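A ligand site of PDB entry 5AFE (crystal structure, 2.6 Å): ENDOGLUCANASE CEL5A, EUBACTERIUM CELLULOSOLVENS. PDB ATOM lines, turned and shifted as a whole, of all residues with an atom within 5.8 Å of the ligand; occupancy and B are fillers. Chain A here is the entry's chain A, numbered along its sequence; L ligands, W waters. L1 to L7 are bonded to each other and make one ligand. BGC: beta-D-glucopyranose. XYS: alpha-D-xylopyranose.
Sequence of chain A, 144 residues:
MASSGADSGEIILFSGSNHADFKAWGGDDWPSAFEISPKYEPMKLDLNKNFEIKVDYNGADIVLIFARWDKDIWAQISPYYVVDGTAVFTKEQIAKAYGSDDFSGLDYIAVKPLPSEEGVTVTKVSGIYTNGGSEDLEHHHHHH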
ATOM      1  N   TRP A  25       4.490  12.047  -5.312  1.00  0.00           N
ATOM      2  CA  TRP A  25       5.227  12.088  -4.035  1.00  0.00           C
ATOM      3  C   TRP A  25       6.666  11.628  -4.232  1.00  0.00           C
ATOM      4  O   TRP A  25       7.045  11.169  -5.310  1.00  0.00           O
ATOM      5  CB  TRP A  25       4.520  11.220  -2.967  1.00  0.00           C
ATOM      6  CG  TRP A  25       3.305  11.870  -2.374  1.00  0.00           C
ATOM      7  CD1 TRP A  25       3.264  12.978  -1.593  1.00  0.00           C
ATOM      8  CD2 TRP A  25       1.944  11.425  -2.520  1.00  0.00           C
ATOM      9  NE1 TRP A  25       1.965  13.273  -1.248  1.00  0.00           N
ATOM     10  CE2 TRP A  25       1.133  12.336  -1.803  1.00  0.00           C
ATOM     11  CE3 TRP A  25       1.337  10.356  -3.185  1.00  0.00           C
ATOM     12  CZ2 TRP A  25      -0.255  12.207  -1.731  1.00  0.00           C
ATOM     13  CZ3 TRP A  25      -0.051  10.227  -3.113  1.00  0.00           C
ATOM     14  CH2 TRP A  25      -0.829  11.147  -2.384  1.00  0.00           C
ATOM     15  N   GLY A  26       7.466  11.771  -3.175  1.00  0.00           N
ATOM     16  CA  GLY A  26       8.857  11.324  -3.180  1.00  0.00           C
ATOM     17  C   GLY A  26       9.849  12.360  -3.677  1.00  0.00           C
ATOM     18  O   GLY A  26      11.019  12.039  -3.889  1.00  0.00           O
ATOM     19  N   GLY A  27       9.388  13.598  -3.844  1.00  0.00           N
ATOM     20  CA  GLY A  27      10.251  14.713  -4.252  1.00  0.00           C
ATOM     21  C   GLY A  27      10.699  15.527  -3.056  1.00  0.00           C
ATOM     22  O   GLY A  27      10.783  15.015  -1.947  1.00  0.00           O
ATOM     23  N   ASP A  28      10.978  16.803  -3.296  1.00  0.00           N
ATOM     24  CA  ASP A  28      11.427  17.711  -2.233  1.00  0.00           C
ATOM     25  C   ASP A  28      10.270  18.210  -1.395  1.00  0.00           C
ATOM     26  O   ASP A  28      10.228  17.976  -0.178  1.00  0.00           O
ATOM     27  CB  ASP A  28      12.163  18.923  -2.834  1.00  0.00           C
ATOM     28  CG  ASP A  28      13.444  18.543  -3.538  1.00  0.00           C
ATOM     29  OD1 ASP A  28      14.369  18.047  -2.875  1.00  0.00           O
ATOM     30  OD2 ASP A  28      13.511  18.761  -4.768  1.00  0.00           O
ATOM     31  N   ASP A  29       9.326  18.879  -2.040  1.00  0.00           N
ATOM     32  CA  ASP A  29       8.237  19.596  -1.370  1.00  0.00           C
ATOM     33  C   ASP A  29       6.882  19.176  -1.926  1.00  0.00           C
ATOM     34  O   ASP A  29       6.744  18.952  -3.122  1.00  0.00           O
ATOM     35  CB  ASP A  29       8.441  21.113  -1.562  1.00  0.00           C
ATOM     36  CG  ASP A  29       7.264  21.938  -1.035  1.00  0.00           C
ATOM     37  OD1 ASP A  29       6.716  21.608   0.041  1.00  0.00           O
ATOM     38  OD2 ASP A  29       6.891  22.927  -1.702  1.00  0.00           O
ATOM     39  N   TRP A  30       5.897  19.057  -1.039  1.00  0.00           N
ATOM     40  CA  TRP A  30       4.503  18.866  -1.416  1.00  0.00           C
ATOM     41  C   TRP A  30       3.777  20.200  -1.229  1.00  0.00           C
ATOM     42  O   TRP A  30       3.371  20.529  -0.115  1.00  0.00           O
ATOM     43  CB  TRP A  30       3.867  17.756  -0.574  1.00  0.00           C
ATOM     44  CG  TRP A  30       2.417  17.458  -0.895  1.00  0.00           C
ATOM     45  CD1 TRP A  30       1.733  17.811  -2.027  1.00  0.00           C
ATOM     46  CD2 TRP A  30       1.492  16.709  -0.094  1.00  0.00           C
ATOM     47  NE1 TRP A  30       0.434  17.348  -1.968  1.00  0.00           N
ATOM     48  CE2 TRP A  30       0.262  16.662  -0.793  1.00  0.00           C
ATOM     49  CE3 TRP A  30       1.579  16.073   1.152  1.00  0.00           C
ATOM     50  CZ2 TRP A  30      -0.868  16.011  -0.294  1.00  0.00           C
ATOM     51  CZ3 TRP A  30       0.451  15.436   1.653  1.00  0.00           C
ATOM     52  CH2 TRP A  30      -0.751  15.409   0.931  1.00  0.00           C
ATOM     53  N   PRO A  31       3.629  20.990  -2.308  1.00  0.00           N
ATOM     54  CA  PRO A  31       3.114  22.361  -2.190  1.00  0.00           C
ATOM     55  C   PRO A  31       1.617  22.467  -1.912  1.00  0.00           C
ATOM     56  O   PRO A  31       0.853  21.541  -2.205  1.00  0.00           O
ATOM     57  CB  PRO A  31       3.441  22.975  -3.548  1.00  0.00           C
ATOM     58  CG  PRO A  31       3.429  21.835  -4.484  1.00  0.00           C
ATOM     59  CD  PRO A  31       3.965  20.667  -3.707  1.00  0.00           C
ATOM     60  N   SER A  32       1.213  23.622  -1.361  1.00  0.00           N
ATOM     61  CA  SER A  32      -0.172  23.913  -1.004  1.00  0.00           C
ATOM     62  C   SER A  32      -0.726  25.030  -1.889  1.00  0.00           C
ATOM     63  O   SER A  32      -0.010  25.972  -2.241  1.00  0.00           O
ATOM     64  CB  SER A  32      -0.258  24.374   0.455  1.00  0.00           C
ATOM     65  OG  SER A  32       0.589  23.602   1.297  1.00  0.00           O
ATOM     66  N   GLU A  35      -2.442  27.861   2.691  1.00  0.00           N
ATOM     67  CA  GLU A  35      -1.885  27.381   3.958  1.00  0.00           C
ATOM     68  C   GLU A  35      -1.674  28.481   5.016  1.00  0.00           C
ATOM     69  O   GLU A  35      -1.392  29.631   4.671  1.00  0.00           O
ATOM     70  CB  GLU A  35      -0.554  26.676   3.707  1.00  0.00           C
ATOM     71  CG  GLU A  35       0.410  27.477   2.853  1.00  0.00           C
ATOM     72  CD  GLU A  35       1.841  26.966   2.921  1.00  0.00           C
ATOM     73  OE1 GLU A  35       2.056  25.862   3.460  1.00  0.00           O
ATOM     74  OE2 GLU A  35       2.740  27.670   2.418  1.00  0.00           O
ATOM     75  N   TRP A  69       3.800  19.600  14.770  1.00  0.00           N
ATOM     76  CA  TRP A  69       5.129  19.013  14.564  1.00  0.00           C
ATOM     77  C   TRP A  69       5.681  18.259  15.783  1.00  0.00           C
ATOM     78  O   TRP A  69       6.254  17.180  15.625  1.00  0.00           O
ATOM     79  CB  TRP A  69       6.153  20.091  14.160  1.00  0.00           C
ATOM     80  CG  TRP A  69       5.756  21.028  13.034  1.00  0.00           C
ATOM     81  CD1 TRP A  69       5.929  22.386  13.017  1.00  0.00           C
ATOM     82  CD2 TRP A  69       5.148  20.687  11.785  1.00  0.00           C
ATOM     83  NE1 TRP A  69       5.469  22.907  11.837  1.00  0.00           N
ATOM     84  CE2 TRP A  69       4.978  21.885  11.056  1.00  0.00           C
ATOM     85  CE3 TRP A  69       4.726  19.484  11.190  1.00  0.00           C
ATOM     86  CZ2 TRP A  69       4.410  21.930   9.778  1.00  0.00           C
ATOM     87  CZ3 TRP A  69       4.152  19.521   9.915  1.00  0.00           C
ATOM     88  CH2 TRP A  69       4.003  20.741   9.228  1.00  0.00           C
ATOM     89  N   ASP A  72       3.803  15.342  16.451  1.00  0.00           N
ATOM     90  CA  ASP A  72       3.983  14.682  15.164  1.00  0.00           C
ATOM     91  C   ASP A  72       2.665  14.092  14.671  1.00  0.00           C
ATOM     92  O   ASP A  72       2.533  12.890  14.474  1.00  0.00           O
ATOM     93  CB  ASP A  72       5.090  13.611  15.238  1.00  0.00           C
ATOM     94  CG  ASP A  72       5.811  13.415  13.907  1.00  0.00           C
ATOM     95  OD1 ASP A  72       5.256  13.779  12.836  1.00  0.00           O
ATOM     96  OD2 ASP A  72       6.944  12.900  13.924  1.00  0.00           O
ATOM     97  N   TRP A  74      -0.391  14.378  11.664  1.00  0.00           N
ATOM     98  CA  TRP A  74      -0.683  14.798  10.295  1.00  0.00           C
ATOM     99  C   TRP A  74      -2.068  14.302   9.933  1.00  0.00           C
ATOM    100  O   TRP A  74      -2.226  13.298   9.230  1.00  0.00           O
ATOM    101  CB  TRP A  74       0.385  14.260   9.336  1.00  0.00           C
ATOM    102  CG  TRP A  74       0.276  14.750   7.889  1.00  0.00           C
ATOM    103  CD1 TRP A  74      -0.515  14.231   6.902  1.00  0.00           C
ATOM    104  CD2 TRP A  74       1.039  15.801   7.279  1.00  0.00           C
ATOM    105  NE1 TRP A  74      -0.308  14.913   5.721  1.00  0.00           N
ATOM    106  CE2 TRP A  74       0.639  15.874   5.929  1.00  0.00           C
ATOM    107  CE3 TRP A  74       2.010  16.693   7.744  1.00  0.00           C
ATOM    108  CZ2 TRP A  74       1.177  16.808   5.041  1.00  0.00           C
ATOM    109  CZ3 TRP A  74       2.542  17.620   6.861  1.00  0.00           C
ATOM    110  CH2 TRP A  74       2.124  17.673   5.523  1.00  0.00           C
ATOM    111  N   GLN A  76      -5.098  14.354   7.808  1.00  0.00           N
ATOM    112  CA  GLN A  76      -5.265  14.639   6.397  1.00  0.00           C
ATOM    113  C   GLN A  76      -6.556  13.979   5.974  1.00  0.00           C
ATOM    114  O   GLN A  76      -6.718  12.774   6.160  1.00  0.00           O
ATOM    115  CB  GLN A  76      -4.079  14.050   5.621  1.00  0.00           C
ATOM    116  CG  GLN A  76      -4.197  14.097   4.104  1.00  0.00           C
ATOM    117  CD  GLN A  76      -3.009  13.455   3.412  1.00  0.00           C
ATOM    118  OE1 GLN A  76      -1.852  13.732   3.758  1.00  0.00           O
ATOM    119  NE2 GLN A  76      -3.277  12.582   2.451  1.00  0.00           N
ATOM    120  N   TYR A 108      -0.001  23.958  11.836  1.00  0.00           N
ATOM    121  CA  TYR A 108      -0.109  24.038  10.389  1.00  0.00           C
ATOM    122  C   TYR A 108      -1.471  23.615   9.867  1.00  0.00           C
ATOM    123  O   TYR A 108      -2.038  22.614  10.313  1.00  0.00           O
ATOM    124  CB  TYR A 108       0.992  23.167   9.796  1.00  0.00           C
ATOM    125  CG  TYR A 108       1.137  23.227   8.295  1.00  0.00           C
ATOM    126  CD1 TYR A 108       1.647  24.357   7.667  1.00  0.00           C
ATOM    127  CD2 TYR A 108       0.795  22.128   7.507  1.00  0.00           C
ATOM    128  CE1 TYR A 108       1.793  24.402   6.289  1.00  0.00           C
ATOM    129  CE2 TYR A 108       0.932  22.161   6.120  1.00  0.00           C
ATOM    130  CZ  TYR A 108       1.431  23.305   5.520  1.00  0.00           C
ATOM    131  OH  TYR A 108       1.569  23.329   4.144  1.00  0.00           O
ATOM    132  N   LYS A 112      -4.119  20.996  -0.022  1.00  0.00           N
ATOM    133  CA  LYS A 112      -3.091  20.446  -0.890  1.00  0.00           C
ATOM    134  C   LYS A 112      -3.699  19.531  -1.955  1.00  0.00           C
ATOM    135  O   LYS A 112      -4.654  18.816  -1.670  1.00  0.00           O
ATOM    136  CB  LYS A 112      -2.078  19.653  -0.059  1.00  0.00           C
ATOM    137  CG  LYS A 112      -1.209  20.525   0.827  1.00  0.00           C
ATOM    138  CD  LYS A 112      -0.266  19.656   1.650  1.00  0.00           C
ATOM    139  CE  LYS A 112       0.686  20.500   2.491  1.00  0.00           C
ATOM    140  NZ  LYS A 112       1.575  21.345   1.650  1.00  0.00           N
HETATM  141  C2  BGC L   1       8.561  22.143   7.958  1.00  0.00           C
HETATM  142  C3  BGC L   1       7.769  20.844   7.827  1.00  0.00           C
HETATM  143  C4  BGC L   1       8.429  19.708   8.618  1.00  0.00           C
HETATM  144  C5  BGC L   1       8.812  20.146  10.040  1.00  0.00           C
HETATM  145  C6  BGC L   1       9.717  19.105  10.716  1.00  0.00           C
HETATM  146  C1  BGC L   1       8.756  22.457   9.433  1.00  0.00           C
HETATM  147  O1  BGC L   1       9.471  23.695   9.567  1.00  0.00           O
HETATM  148  O2  BGC L   1       7.887  23.223   7.294  1.00  0.00           O
HETATM  149  O3  BGC L   1       7.691  20.505   6.430  1.00  0.00           O
HETATM  150  O4  BGC L   1       7.545  18.579   8.733  1.00  0.00           O
HETATM  151  O5  BGC L   1       9.499  21.396  10.035  1.00  0.00           O
HETATM  152  O6  BGC L   1       9.057  18.532  11.855  1.00  0.00           O
HETATM  153  C2  BGC L   2       7.137  16.284   8.067  1.00  0.00           C
HETATM  154  C3  BGC L   2       6.907  15.305   6.915  1.00  0.00           C
HETATM  155  C4  BGC L   2       6.347  15.951   5.650  1.00  0.00           C
HETATM  156  C5  BGC L   2       7.060  17.272   5.367  1.00  0.00           C
HETATM  157  C6  BGC L   2       6.554  18.036   4.135  1.00  0.00           C
HETATM  158  C1  BGC L   2       7.654  17.657   7.633  1.00  0.00           C
HETATM  159  O2  BGC L   2       8.099  15.685   8.952  1.00  0.00           O
HETATM  160  O3  BGC L   2       6.014  14.284   7.362  1.00  0.00           O
HETATM  161  O4  BGC L   2       6.542  15.036   4.568  1.00  0.00           O
HETATM  162  O5  BGC L   2       6.906  18.111   6.504  1.00  0.00           O
HETATM  163  O6  BGC L   2       5.330  18.703   4.456  1.00  0.00           O
HETATM  164  C2  BGC L   3       5.607  13.576   2.879  1.00  0.00           C
HETATM  165  C3  BGC L   3       4.307  13.069   2.261  1.00  0.00           C
HETATM  166  C4  BGC L   3       3.378  12.477   3.317  1.00  0.00           C
HETATM  167  C5  BGC L   3       3.311  13.309   4.594  1.00  0.00           C
HETATM  168  C6  BGC L   3       2.545  12.563   5.679  1.00  0.00           C
HETATM  169  C1  BGC L   3       5.312  14.476   4.082  1.00  0.00           C
HETATM  170  O2  BGC L   3       6.351  14.299   1.893  1.00  0.00           O
HETATM  171  O3  BGC L   3       4.605  12.070   1.285  1.00  0.00           O
HETATM  172  O4  BGC L   3       2.042  12.381   2.794  1.00  0.00           O
HETATM  173  O5  BGC L   3       4.621  13.690   5.043  1.00  0.00           O
HETATM  174  O6  BGC L   3       3.395  12.102   6.750  1.00  0.00           O
HETATM  175  C1  XYS L   4       4.719  19.601   3.488  1.00  0.00           C
HETATM  176  C2  XYS L   4       5.620  20.465   2.598  1.00  0.00           C
HETATM  177  C3  XYS L   4       6.352  21.579   3.350  1.00  0.00           C
HETATM  178  C4  XYS L   4       5.450  22.305   4.351  1.00  0.00           C
HETATM  179  C5  XYS L   4       4.557  21.340   5.110  1.00  0.00           C
HETATM  180  O2  XYS L   4       6.564  19.660   1.862  1.00  0.00           O
HETATM  181  O3  XYS L   4       6.826  22.550   2.406  1.00  0.00           O
HETATM  182  O4  XYS L   4       6.255  23.037   5.278  1.00  0.00           O
HETATM  183  O5  XYS L   4       3.850  20.494   4.186  1.00  0.00           O
HETATM  184  C2  BGC L   5       0.158  10.953   2.319  1.00  0.00           C
HETATM  185  C3  BGC L   5      -0.332   9.636   1.677  1.00  0.00           C
HETATM  186  C4  BGC L   5       0.614   9.047   0.625  1.00  0.00           C
HETATM  187  C5  BGC L   5       2.063   9.243   1.020  1.00  0.00           C
HETATM  188  C6  BGC L   5       3.061   8.731  -0.021  1.00  0.00           C
HETATM  189  C1  BGC L   5       1.683  11.046   2.459  1.00  0.00           C
HETATM  190  O2  BGC L   5      -0.421  11.075   3.635  1.00  0.00           O
HETATM  191  O3  BGC L   5      -1.603   9.879   1.061  1.00  0.00           O
HETATM  192  O4  BGC L   5       0.365   7.643   0.506  1.00  0.00           O
HETATM  193  O5  BGC L   5       2.303  10.628   1.242  1.00  0.00           O
HETATM  194  O6  BGC L   5       4.219   8.345   0.726  1.00  0.00           O
HETATM  195  C1  XYS L   6       4.144  10.911   6.421  1.00  0.00           C
HETATM  196  C2  XYS L   6       3.304   9.650   6.574  1.00  0.00           C
HETATM  197  C3  XYS L   6       2.805   9.582   8.006  1.00  0.00           C
HETATM  198  C4  XYS L   6       3.988   9.563   8.962  1.00  0.00           C
HETATM  199  C5  XYS L   6       4.991  10.675   8.657  1.00  0.00           C
HETATM  200  O2  XYS L   6       2.193   9.595   5.672  1.00  0.00           O
HETATM  201  O3  XYS L   6       1.990   8.405   8.141  1.00  0.00           O
HETATM  202  O4  XYS L   6       3.524   9.707  10.314  1.00  0.00           O
HETATM  203  O5  XYS L   6       5.287  10.767   7.258  1.00  0.00           O
HETATM  204  C1  XYS L   7       5.445   8.597   0.021  1.00  0.00           C
HETATM  205  C2  XYS L   7       5.712   7.374  -0.840  1.00  0.00           C
HETATM  206  C3  XYS L   7       7.095   7.442  -1.502  1.00  0.00           C
HETATM  207  C4  XYS L   7       7.805   8.750  -1.161  1.00  0.00           C
HETATM  208  C5  XYS L   7       7.787   9.076   0.339  1.00  0.00           C
HETATM  209  O2  XYS L   7       5.615   6.208  -0.012  1.00  0.00           O
HETATM  210  O3  XYS L   7       6.974   7.342  -2.926  1.00  0.00           O
HETATM  211  O4  XYS L   7       9.155   8.640  -1.610  1.00  0.00           O
HETATM  212  O5  XYS L   7       6.513   8.805   0.945  1.00  0.00           O
HETATM  213  O   HOH W   1      -0.019   8.218   5.770  1.00  0.00           O
HETATM  214  O   HOH W   2       9.091  18.890   2.146  1.00  0.00           O
HETATM  215  O   HOH W   3      12.284  22.358  10.127  1.00  0.00           O
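The side-chain carboxylate (OD1) of Asp 29 lies within hydrogen-bond range of an oxygen (O3) of XYS L4, at 2.5 Å. OE1 of Gln 76 lies within hydrogen-bond range of O2 of BGC L5 (3.0 Å). N of Trp 30 sits at hydrogen-bond distance from O2 of XYS L4.
OE1 of Gln 76 lies within hydrogen-bond range of NE1 of Trp 74 (2.8 Å). NZ of Lys 112 lies within hydrogen-bond range of O of Trp 30 (2.6 Å). NZ of Lys 112 sits at hydrogen-bond distance from OH of Tyr 108. OG of Ser 32 lies within hydrogen-bond range of NZ of Lys 112 (2.5 Å). OH of Tyr 108 lies within hydrogen-bond range of OE1 of Glu 35, at 2.7 Å. The side-chain hydroxyl of Ser 32 sits at hydrogen-bond distance from the side-chain hydroxyl of Tyr 108, at 3.0 Å.
Residues that only touch the ligand: Trp 25 (3.3 Å), Gly 26 (3.1 Å), Trp 69 (3.7 Å), Trp 74 (3.5 Å), Tyr 108 (3.6 Å) and Lys 112 (3.5 Å). Hydrophobic or aromatic side chains within 4 Å of the ligand: Trp 25, Trp 30, Trp 69, Trp 74 and Tyr 108. The nearest printed residue that does not touch the ligand is Asp 28 (4.5 Å).
Water W2 lies within hydrogen-bond range of an oxygen (O2) of XYS L4 (2.7 Å) and the backbone carbonyl oxygen (O) of Asp 28 (2.7 Å).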
